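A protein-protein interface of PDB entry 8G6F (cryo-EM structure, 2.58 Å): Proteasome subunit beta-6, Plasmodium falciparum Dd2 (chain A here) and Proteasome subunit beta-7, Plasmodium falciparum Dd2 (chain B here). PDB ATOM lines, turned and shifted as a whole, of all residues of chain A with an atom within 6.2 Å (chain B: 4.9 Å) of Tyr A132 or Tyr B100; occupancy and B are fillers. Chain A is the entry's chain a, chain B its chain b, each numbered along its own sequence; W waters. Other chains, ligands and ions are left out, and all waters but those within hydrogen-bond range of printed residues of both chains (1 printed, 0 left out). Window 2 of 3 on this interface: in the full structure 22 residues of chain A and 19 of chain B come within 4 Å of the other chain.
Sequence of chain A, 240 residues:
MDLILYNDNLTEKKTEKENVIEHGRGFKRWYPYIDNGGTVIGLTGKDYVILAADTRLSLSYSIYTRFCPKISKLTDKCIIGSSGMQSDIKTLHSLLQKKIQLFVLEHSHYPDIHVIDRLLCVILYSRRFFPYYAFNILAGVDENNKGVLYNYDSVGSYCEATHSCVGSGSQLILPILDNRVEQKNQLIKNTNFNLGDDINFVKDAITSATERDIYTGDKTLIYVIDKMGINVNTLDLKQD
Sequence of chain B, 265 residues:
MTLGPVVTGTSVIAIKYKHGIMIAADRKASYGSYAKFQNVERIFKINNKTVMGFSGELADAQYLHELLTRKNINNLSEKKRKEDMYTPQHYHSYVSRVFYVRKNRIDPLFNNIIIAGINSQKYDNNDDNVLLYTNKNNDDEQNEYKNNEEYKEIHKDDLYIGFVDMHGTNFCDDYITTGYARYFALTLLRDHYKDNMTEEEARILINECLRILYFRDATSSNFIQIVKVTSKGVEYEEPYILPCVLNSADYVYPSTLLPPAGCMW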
ATOM      1  N   TYR A  33     -24.621  -5.897  16.455  1.00  0.00           N
ATOM      2  CA  TYR A  33     -23.705  -6.549  15.533  1.00  0.00           C
ATOM      3  C   TYR A  33     -24.325  -7.822  14.984  1.00  0.00           C
ATOM      4  O   TYR A  33     -24.931  -8.599  15.724  1.00  0.00           O
ATOM      5  CB  TYR A  33     -22.385  -6.904  16.205  1.00  0.00           C
ATOM      6  CG  TYR A  33     -21.583  -5.722  16.668  1.00  0.00           C
ATOM      7  CD1 TYR A  33     -20.863  -4.957  15.772  1.00  0.00           C
ATOM      8  CD2 TYR A  33     -21.535  -5.381  18.005  1.00  0.00           C
ATOM      9  CE1 TYR A  33     -20.125  -3.885  16.193  1.00  0.00           C
ATOM     10  CE2 TYR A  33     -20.803  -4.309  18.434  1.00  0.00           C
ATOM     11  CZ  TYR A  33     -20.097  -3.565  17.526  1.00  0.00           C
ATOM     12  OH  TYR A  33     -19.359  -2.490  17.954  1.00  0.00           O
ATOM     13  N   SER A  87     -23.691  -3.580   6.567  1.00  0.00           N
ATOM     14  CA  SER A  87     -23.935  -2.150   6.712  1.00  0.00           C
ATOM     15  C   SER A  87     -22.664  -1.411   7.109  1.00  0.00           C
ATOM     16  O   SER A  87     -22.365  -0.338   6.571  1.00  0.00           O
ATOM     17  CB  SER A  87     -25.037  -1.915   7.738  1.00  0.00           C
ATOM     18  OG  SER A  87     -24.674  -2.430   8.999  1.00  0.00           O
ATOM     19  N   ASP A  88     -21.899  -1.977   8.042  1.00  0.00           N
ATOM     20  CA  ASP A  88     -20.627  -1.375   8.416  1.00  0.00           C
ATOM     21  C   ASP A  88     -19.668  -1.347   7.235  1.00  0.00           C
ATOM     22  O   ASP A  88     -18.966  -0.355   7.024  1.00  0.00           O
ATOM     23  CB  ASP A  88     -20.008  -2.142   9.582  1.00  0.00           C
ATOM     24  CG  ASP A  88     -20.489  -1.648  10.923  1.00  0.00           C
ATOM     25  OD1 ASP A  88     -21.343  -0.745  10.958  1.00  0.00           O
ATOM     26  OD2 ASP A  88     -20.010  -2.160  11.950  1.00  0.00           O
ATOM     27  N   ILE A  89     -19.623  -2.428   6.459  1.00  0.00           N
ATOM     28  CA  ILE A  89     -18.723  -2.485   5.311  1.00  0.00           C
ATOM     29  C   ILE A  89     -19.092  -1.412   4.296  1.00  0.00           C
ATOM     30  O   ILE A  89     -18.229  -0.703   3.771  1.00  0.00           O
ATOM     31  CB  ILE A  89     -18.754  -3.886   4.678  1.00  0.00           C
ATOM     32  CG1 ILE A  89     -18.155  -4.914   5.633  1.00  0.00           C
ATOM     33  CG2 ILE A  89     -18.012  -3.891   3.356  1.00  0.00           C
ATOM     34  CD1 ILE A  89     -18.633  -6.302   5.378  1.00  0.00           C
ATOM     35  N   THR A  91     -20.816   1.409   4.755  1.00  0.00           N
ATOM     36  CA  THR A  91     -20.534   2.741   5.271  1.00  0.00           C
ATOM     37  C   THR A  91     -19.042   3.030   5.258  1.00  0.00           C
ATOM     38  O   THR A  91     -18.624   4.130   4.894  1.00  0.00           O
ATOM     39  CB  THR A  91     -21.096   2.883   6.682  1.00  0.00           C
ATOM     40  OG1 THR A  91     -22.527   2.868   6.625  1.00  0.00           O
ATOM     41  CG2 THR A  91     -20.628   4.179   7.317  1.00  0.00           C
ATOM     42  N   LEU A  92     -18.220   2.057   5.651  1.00  0.00           N
ATOM     43  CA  LEU A  92     -16.783   2.281   5.708  1.00  0.00           C
ATOM     44  C   LEU A  92     -16.195   2.479   4.317  1.00  0.00           C
ATOM     45  O   LEU A  92     -15.345   3.350   4.117  1.00  0.00           O
ATOM     46  CB  LEU A  92     -16.109   1.110   6.419  1.00  0.00           C
ATOM     47  CG  LEU A  92     -14.601   1.209   6.629  1.00  0.00           C
ATOM     48  CD1 LEU A  92     -14.278   2.199   7.729  1.00  0.00           C
ATOM     49  CD2 LEU A  92     -14.037  -0.154   6.951  1.00  0.00           C
ATOM     50  N   LEU A  95     -17.196   5.906   3.152  1.00  0.00           N
ATOM     51  CA  LEU A  95     -16.438   6.928   3.864  1.00  0.00           C
ATOM     52  C   LEU A  95     -15.018   7.030   3.333  1.00  0.00           C
ATOM     53  O   LEU A  95     -14.489   8.131   3.153  1.00  0.00           O
ATOM     54  CB  LEU A  95     -16.428   6.613   5.358  1.00  0.00           C
ATOM     55  CG  LEU A  95     -15.967   7.712   6.310  1.00  0.00           C
ATOM     56  CD1 LEU A  95     -16.649   9.037   6.016  1.00  0.00           C
ATOM     57  CD2 LEU A  95     -16.229   7.283   7.731  1.00  0.00           C
ATOM     58  N   ILE A 123      -9.392   6.282  10.298  1.00  0.00           N
ATOM     59  CA  ILE A 123     -10.842   6.104  10.270  1.00  0.00           C
ATOM     60  C   ILE A 123     -11.260   4.988  11.216  1.00  0.00           C
ATOM     61  O   ILE A 123     -12.276   5.091  11.913  1.00  0.00           O
ATOM     62  CB  ILE A 123     -11.320   5.821   8.834  1.00  0.00           C
ATOM     63  CG1 ILE A 123     -11.252   7.089   7.988  1.00  0.00           C
ATOM     64  CG2 ILE A 123     -12.729   5.253   8.846  1.00  0.00           C
ATOM     65  CD1 ILE A 123     -11.473   6.849   6.513  1.00  0.00           C
ATOM     66  N   LEU A 124     -10.502   3.896  11.240  1.00  0.00           N
ATOM     67  CA  LEU A 124     -10.897   2.735  12.022  1.00  0.00           C
ATOM     68  C   LEU A 124     -10.682   2.961  13.511  1.00  0.00           C
ATOM     69  O   LEU A 124     -11.518   2.556  14.322  1.00  0.00           O
ATOM     70  CB  LEU A 124     -10.125   1.503  11.557  1.00  0.00           C
ATOM     71  CG  LEU A 124     -10.589   0.887  10.238  1.00  0.00           C
ATOM     72  CD1 LEU A 124      -9.707  -0.283   9.874  1.00  0.00           C
ATOM     73  CD2 LEU A 124     -12.034   0.456  10.316  1.00  0.00           C
ATOM     74  N   SER A 126     -10.822   5.801  14.953  1.00  0.00           N
ATOM     75  CA  SER A 126     -11.764   6.810  15.427  1.00  0.00           C
ATOM     76  C   SER A 126     -12.947   6.175  16.148  1.00  0.00           C
ATOM     77  O   SER A 126     -13.500   6.775  17.075  1.00  0.00           O
ATOM     78  CB  SER A 126     -12.250   7.663  14.259  1.00  0.00           C
ATOM     79  OG  SER A 126     -13.379   7.082  13.640  1.00  0.00           O
ATOM     80  N   ARG A 127     -13.343   4.970  15.747  1.00  0.00           N
ATOM     81  CA  ARG A 127     -14.435   4.233  16.373  1.00  0.00           C
ATOM     82  C   ARG A 127     -13.901   3.099  17.245  1.00  0.00           C
ATOM     83  O   ARG A 127     -14.496   2.028  17.337  1.00  0.00           O
ATOM     84  CB  ARG A 127     -15.391   3.694  15.313  1.00  0.00           C
ATOM     85  CG  ARG A 127     -16.551   4.618  15.006  1.00  0.00           C
ATOM     86  CD  ARG A 127     -17.554   3.968  14.080  1.00  0.00           C
ATOM     87  NE  ARG A 127     -18.135   2.759  14.647  1.00  0.00           N
ATOM     88  CZ  ARG A 127     -19.103   2.056  14.077  1.00  0.00           C
ATOM     89  NH1 ARG A 127     -19.629   2.414  12.920  1.00  0.00           N
ATOM     90  NH2 ARG A 127     -19.552   0.962  14.684  1.00  0.00           N
ATOM     91  N   PHE A 130     -16.315   1.417  19.640  1.00  0.00           N
ATOM     92  CA  PHE A 130     -17.496   0.830  19.025  1.00  0.00           C
ATOM     93  C   PHE A 130     -17.093   0.419  17.615  1.00  0.00           C
ATOM     94  O   PHE A 130     -17.612   0.959  16.633  1.00  0.00           O
ATOM     95  CB  PHE A 130     -18.663   1.817  19.007  1.00  0.00           C
ATOM     96  CG  PHE A 130     -19.991   1.183  18.708  1.00  0.00           C
ATOM     97  CD1 PHE A 130     -20.499   0.187  19.520  1.00  0.00           C
ATOM     98  CD2 PHE A 130     -20.735   1.589  17.616  1.00  0.00           C
ATOM     99  CE1 PHE A 130     -21.718  -0.390  19.245  1.00  0.00           C
ATOM    100  CE2 PHE A 130     -21.955   1.013  17.339  1.00  0.00           C
ATOM    101  CZ  PHE A 130     -22.448   0.024  18.152  1.00  0.00           C
ATOM    102  N   PRO A 131     -16.174  -0.534  17.479  1.00  0.00           N
ATOM    103  CA  PRO A 131     -15.488  -0.724  16.197  1.00  0.00           C
ATOM    104  C   PRO A 131     -16.425  -1.119  15.068  1.00  0.00           C
ATOM    105  O   PRO A 131     -17.466  -1.744  15.276  1.00  0.00           O
ATOM    106  CB  PRO A 131     -14.489  -1.849  16.496  1.00  0.00           C
ATOM    107  CG  PRO A 131     -14.371  -1.889  17.964  1.00  0.00           C
ATOM    108  CD  PRO A 131     -15.684  -1.465  18.504  1.00  0.00           C
ATOM    109  N   TYR A 132     -16.040  -0.731  13.853  1.00  0.00           N
ATOM    110  CA  TYR A 132     -16.651  -1.299  12.663  1.00  0.00           C
ATOM    111  C   TYR A 132     -16.486  -2.809  12.692  1.00  0.00           C
ATOM    112  O   TYR A 132     -15.382  -3.317  12.897  1.00  0.00           O
ATOM    113  CB  TYR A 132     -15.994  -0.743  11.401  1.00  0.00           C
ATOM    114  CG  TYR A 132     -16.286   0.701  11.093  1.00  0.00           C
ATOM    115  CD1 TYR A 132     -17.446   1.069  10.435  1.00  0.00           C
ATOM    116  CD2 TYR A 132     -15.384   1.696  11.435  1.00  0.00           C
ATOM    117  CE1 TYR A 132     -17.709   2.385  10.143  1.00  0.00           C
ATOM    118  CE2 TYR A 132     -15.636   3.012  11.145  1.00  0.00           C
ATOM    119  CZ  TYR A 132     -16.800   3.354  10.502  1.00  0.00           C
ATOM    120  OH  TYR A 132     -17.053   4.672  10.214  1.00  0.00           O
ATOM    121  N   TYR A 133     -17.581  -3.533  12.476  1.00  0.00           N
ATOM    122  CA  TYR A 133     -17.515  -4.987  12.387  1.00  0.00           C
ATOM    123  C   TYR A 133     -17.149  -5.342  10.950  1.00  0.00           C
ATOM    124  O   TYR A 133     -17.979  -5.745  10.135  1.00  0.00           O
ATOM    125  CB  TYR A 133     -18.831  -5.620  12.818  1.00  0.00           C
ATOM    126  CG  TYR A 133     -18.772  -7.123  12.989  1.00  0.00           C
ATOM    127  CD1 TYR A 133     -17.588  -7.824  12.799  1.00  0.00           C
ATOM    128  CD2 TYR A 133     -19.901  -7.841  13.343  1.00  0.00           C
ATOM    129  CE1 TYR A 133     -17.536  -9.185  12.952  1.00  0.00           C
ATOM    130  CE2 TYR A 133     -19.854  -9.203  13.500  1.00  0.00           C
ATOM    131  CZ  TYR A 133     -18.670  -9.871  13.305  1.00  0.00           C
ATOM    132  OH  TYR A 133     -18.611 -11.235  13.460  1.00  0.00           O
ATOM    133  N   ALA A 134     -15.869  -5.173  10.639  1.00  0.00           N
ATOM    134  CA  ALA A 134     -15.383  -5.389   9.285  1.00  0.00           C
ATOM    135  C   ALA A 134     -13.899  -5.699   9.334  1.00  0.00           C
ATOM    136  O   ALA A 134     -13.132  -4.962   9.957  1.00  0.00           O
ATOM    137  CB  ALA A 134     -15.642  -4.161   8.409  1.00  0.00           C
ATOM    138  N   PHE A 135     -13.509  -6.790   8.690  1.00  0.00           N
ATOM    139  CA  PHE A 135     -12.115  -7.140   8.474  1.00  0.00           C
ATOM    140  C   PHE A 135     -11.787  -6.860   7.020  1.00  0.00           C
ATOM    141  O   PHE A 135     -12.497  -7.323   6.124  1.00  0.00           O
ATOM    142  CB  PHE A 135     -11.861  -8.606   8.817  1.00  0.00           C
ATOM    143  CG  PHE A 135     -12.294  -8.975  10.196  1.00  0.00           C
ATOM    144  CD1 PHE A 135     -11.447  -8.792  11.270  1.00  0.00           C
ATOM    145  CD2 PHE A 135     -13.558  -9.483  10.425  1.00  0.00           C
ATOM    146  CE1 PHE A 135     -11.847  -9.119  12.543  1.00  0.00           C
ATOM    147  CE2 PHE A 135     -13.963  -9.810  11.696  1.00  0.00           C
ATOM    148  CZ  PHE A 135     -13.106  -9.628  12.756  1.00  0.00           C
ATOM    149  N   ASP A 153      -7.716  -5.724  11.013  1.00  0.00           N
ATOM    150  CA  ASP A 153      -8.512  -6.475  11.970  1.00  0.00           C
ATOM    151  C   ASP A 153      -9.605  -5.622  12.594  1.00  0.00           C
ATOM    152  O   ASP A 153      -9.979  -5.849  13.747  1.00  0.00           O
ATOM    153  CB  ASP A 153      -7.610  -7.063  13.056  1.00  0.00           C
ATOM    154  CG  ASP A 153      -7.117  -6.023  14.038  1.00  0.00           C
ATOM    155  OD1 ASP A 153      -6.209  -5.250  13.683  1.00  0.00           O
ATOM    156  OD2 ASP A 153      -7.624  -5.990  15.174  1.00  0.00           O
ATOM    157  N   SER A 154     -10.125  -4.654  11.844  1.00  0.00           N
ATOM    158  CA  SER A 154     -11.215  -3.785  12.266  1.00  0.00           C
ATOM    159  C   SER A 154     -10.770  -2.638  13.163  1.00  0.00           C
ATOM    160  O   SER A 154     -11.581  -1.764  13.477  1.00  0.00           O
ATOM    161  CB  SER A 154     -12.283  -4.607  12.988  1.00  0.00           C
ATOM    162  OG  SER A 154     -11.887  -4.919  14.311  1.00  0.00           O
ATOM    163  N   VAL A 155      -9.513  -2.621  13.603  1.00  0.00           N
ATOM    164  CA  VAL A 155      -8.970  -1.417  14.227  1.00  0.00           C
ATOM    165  C   VAL A 155      -7.577  -1.050  13.741  1.00  0.00           C
ATOM    166  O   VAL A 155      -7.205   0.134  13.800  1.00  0.00           O
ATOM    167  CB  VAL A 155      -8.981  -1.556  15.764  1.00  0.00           C
ATOM    168  CG1 VAL A 155      -8.378  -0.326  16.414  1.00  0.00           C
ATOM    169  CG2 VAL A 155     -10.395  -1.769  16.260  1.00  0.00           C
ATOM    170  N   SER B  96     -31.709   3.598   4.634  1.00  0.00           N
ATOM    171  CA  SER B  96     -30.557   2.832   5.091  1.00  0.00           C
ATOM    172  C   SER B  96     -29.677   3.665   6.008  1.00  0.00           C
ATOM    173  O   SER B  96     -29.181   3.168   7.023  1.00  0.00           O
ATOM    174  CB  SER B  96     -29.756   2.330   3.895  1.00  0.00           C
ATOM    175  OG  SER B  96     -30.605   1.774   2.914  1.00  0.00           O
ATOM    176  N   ARG B  97     -29.465   4.936   5.664  1.00  0.00           N
ATOM    177  CA  ARG B  97     -28.673   5.808   6.524  1.00  0.00           C
ATOM    178  C   ARG B  97     -29.353   6.017   7.871  1.00  0.00           C
ATOM    179  O   ARG B  97     -28.694   6.011   8.919  1.00  0.00           O
ATOM    180  CB  ARG B  97     -28.434   7.141   5.819  1.00  0.00           C
ATOM    181  CG  ARG B  97     -27.620   8.151   6.600  1.00  0.00           C
ATOM    182  CD  ARG B  97     -26.199   7.689   6.840  1.00  0.00           C
ATOM    183  NE  ARG B  97     -25.505   8.579   7.761  1.00  0.00           N
ATOM    184  CZ  ARG B  97     -24.260   8.406   8.181  1.00  0.00           C
ATOM    185  NH1 ARG B  97     -23.540   7.366   7.800  1.00  0.00           N
ATOM    186  NH2 ARG B  97     -23.726   9.300   9.005  1.00  0.00           N
ATOM    187  N   VAL B  98     -30.674   6.206   7.862  1.00  0.00           N
ATOM    188  CA  VAL B  98     -31.413   6.349   9.115  1.00  0.00           C
ATOM    189  C   VAL B  98     -31.184   5.130   9.999  1.00  0.00           C
ATOM    190  O   VAL B  98     -30.862   5.245  11.190  1.00  0.00           O
ATOM    191  CB  VAL B  98     -32.910   6.555   8.830  1.00  0.00           C
ATOM    192  CG1 VAL B  98     -33.726   6.357  10.095  1.00  0.00           C
ATOM    193  CG2 VAL B  98     -33.160   7.925   8.237  1.00  0.00           C
ATOM    194  N   PHE B  99     -31.349   3.940   9.419  1.00  0.00           N
ATOM    195  CA  PHE B  99     -31.207   2.717  10.196  1.00  0.00           C
ATOM    196  C   PHE B  99     -29.784   2.542  10.700  1.00  0.00           C
ATOM    197  O   PHE B  99     -29.572   2.091  11.828  1.00  0.00           O
ATOM    198  CB  PHE B  99     -31.634   1.518   9.357  1.00  0.00           C
ATOM    199  CG  PHE B  99     -33.097   1.222   9.442  1.00  0.00           C
ATOM    200  CD1 PHE B  99     -34.020   2.085   8.895  1.00  0.00           C
ATOM    201  CD2 PHE B  99     -33.551   0.088  10.079  1.00  0.00           C
ATOM    202  CE1 PHE B  99     -35.359   1.820   8.975  1.00  0.00           C
ATOM    203  CE2 PHE B  99     -34.892  -0.177  10.161  1.00  0.00           C
ATOM    204  CZ  PHE B  99     -35.795   0.688   9.608  1.00  0.00           C
ATOM    205  N   TYR B 100     -28.793   2.889   9.880  1.00  0.00           N
ATOM    206  CA  TYR B 100     -27.406   2.765  10.307  1.00  0.00           C
ATOM    207  C   TYR B 100     -27.114   3.668  11.498  1.00  0.00           C
ATOM    208  O   TYR B 100     -26.471   3.251  12.469  1.00  0.00           O
ATOM    209  CB  TYR B 100     -26.471   3.099   9.147  1.00  0.00           C
ATOM    210  CG  TYR B 100     -25.020   3.070   9.540  1.00  0.00           C
ATOM    211  CD1 TYR B 100     -24.310   1.881   9.553  1.00  0.00           C
ATOM    212  CD2 TYR B 100     -24.362   4.227   9.915  1.00  0.00           C
ATOM    213  CE1 TYR B 100     -22.991   1.849   9.919  1.00  0.00           C
ATOM    214  CE2 TYR B 100     -23.044   4.201  10.285  1.00  0.00           C
ATOM    215  CZ  TYR B 100     -22.363   3.011  10.285  1.00  0.00           C
ATOM    216  OH  TYR B 100     -21.044   2.986  10.652  1.00  0.00           O
ATOM    217  N   VAL B 101     -27.569   4.917  11.437  1.00  0.00           N
ATOM    218  CA  VAL B 101     -27.299   5.840  12.533  1.00  0.00           C
ATOM    219  C   VAL B 101     -27.992   5.371  13.805  1.00  0.00           C
ATOM    220  O   VAL B 101     -27.426   5.440  14.904  1.00  0.00           O
ATOM    221  CB  VAL B 101     -27.721   7.266  12.150  1.00  0.00           C
ATOM    222  CG1 VAL B 101     -27.730   8.154  13.374  1.00  0.00           C
ATOM    223  CG2 VAL B 101     -26.791   7.822  11.097  1.00  0.00           C
ATOM    224  N   ARG B 102     -29.228   4.891  13.682  1.00  0.00           N
ATOM    225  CA  ARG B 102     -29.923   4.409  14.868  1.00  0.00           C
ATOM    226  C   ARG B 102     -29.274   3.149  15.421  1.00  0.00           C
ATOM    227  O   ARG B 102     -29.291   2.932  16.634  1.00  0.00           O
ATOM    228  CB  ARG B 102     -31.392   4.179  14.545  1.00  0.00           C
ATOM    229  CG  ARG B 102     -32.148   5.471  14.381  1.00  0.00           C
ATOM    230  CD  ARG B 102     -33.573   5.234  13.963  1.00  0.00           C
ATOM    231  NE  ARG B 102     -34.470   6.239  14.521  1.00  0.00           N
ATOM    232  CZ  ARG B 102     -34.958   6.204  15.751  1.00  0.00           C
ATOM    233  NH1 ARG B 102     -34.663   5.222  16.585  1.00  0.00           N
ATOM    234  NH2 ARG B 102     -35.761   7.182  16.157  1.00  0.00           N
ATOM    235  N   LYS B 103     -28.689   2.313  14.562  1.00  0.00           N
ATOM    236  CA  LYS B 103     -27.899   1.190  15.053  1.00  0.00           C
ATOM    237  C   LYS B 103     -26.695   1.681  15.843  1.00  0.00           C
ATOM    238  O   LYS B 103     -26.388   1.154  16.917  1.00  0.00           O
ATOM    239  CB  LYS B 103     -27.447   0.314  13.882  1.00  0.00           C
ATOM    240  CG  LYS B 103     -26.365  -0.710  14.215  1.00  0.00           C
ATOM    241  CD  LYS B 103     -25.650  -1.184  12.973  1.00  0.00           C
ATOM    242  CE  LYS B 103     -24.629  -0.174  12.483  1.00  0.00           C
ATOM    243  NZ  LYS B 103     -23.493   0.004  13.424  1.00  0.00           N
ATOM    244  N   ASN B 104     -25.997   2.687  15.320  1.00  0.00           N
ATOM    245  CA  ASN B 104     -24.831   3.208  16.024  1.00  0.00           C
ATOM    246  C   ASN B 104     -25.222   3.753  17.389  1.00  0.00           C
ATOM    247  O   ASN B 104     -24.468   3.621  18.359  1.00  0.00           O
ATOM    248  CB  ASN B 104     -24.154   4.292  15.190  1.00  0.00           C
ATOM    249  CG  ASN B 104     -23.146   3.731  14.217  1.00  0.00           C
ATOM    250  OD1 ASN B 104     -22.889   2.531  14.192  1.00  0.00           O
ATOM    251  ND2 ASN B 104     -22.568   4.600  13.407  1.00  0.00           N
ATOM    252  N   GLY B 168     -29.365  -2.083   9.555  1.00  0.00           N
ATOM    253  CA  GLY B 168     -28.965  -1.273   8.434  1.00  0.00           C
ATOM    254  C   GLY B 168     -28.514  -2.050   7.225  1.00  0.00           C
ATOM    255  O   GLY B 168     -28.124  -1.432   6.228  1.00  0.00           O
HETATM  256  O   HOH W   1     -24.352   5.321   6.510  1.00  0.00           O
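OD1 of Asp A88 is in salt-bridge range of NZ of Lys B103, 3.4 Å away.
NH1 of Arg A127 lies within hydrogen-bond range of OH of Tyr B100.
The guanidinium group (NH2) of Arg A127 lies within hydrogen-bond range of the backbone carbonyl oxygen (O) of Pro A131, at 3.5 Å.
OD2 of Asp A88 lies within hydrogen-bond range of N of Tyr A133 (2.8 Å).
NZ of Lys B103 is in hydrogen-bond range of OD1 of Asn B104, at 2.7 Å.
O of Ser A87 is in hydrogen-bond range of OG1 of Thr A91 (3.2 Å).
NE of Arg A127 is in hydrogen-bond range of O of Phe A130, 2.7 Å away.
Among the printed residues, merely in contact across the chains: Asp A88 with Tyr B100 (3.2 Å), Tyr A132 with Tyr B100 (3.4 Å), Ser A87 with Gly B168 (3.5 Å), Thr A91 with Tyr B100 (3.5 Å), Arg A127 with Asn B104 (3.5 Å) and Phe A130 with Asn B104 (3.6 Å).
Of the printed residues of chain B, Thr A91 touches Tyr B100.
Of the printed residues of chain B, Arg A127 touches Tyr B100 (2.7 Å) and Asn B104 (3.5 Å).
Of chain B, only Tyr B100 (3.4 Å) comes within 4 Å of Tyr A132.
Printed residues of chain A within 4 Å of Gly B168: Ser A87 (3.5 Å).
The nearest residue of chain A that does not touch Tyr B100 is Ser A87 (4.05 Å).
The nearest printed residue of chain A that does not touch Asn B104 is Asp A88 (4.9 Å).
Of the 10 printed residues of chain B, 4 touch a printed residue of chain A.
Hydrophobic or aromatic side chains of chain B within 4 Å of the printed part of chain A: Tyr B100.
Among the printed residues, 8 pairs touch across the chains.
Among the printed residues, Asp or Glu carboxylates within 4 Å of a Lys or Arg side-chain nitrogen of the other chain: Asp A88 with Lys B103 (3.4 Å).
Water W1 bridges NH1 of Arg B97 (2.6 Å) and OG1 of Thr A91 (3.1 Å).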
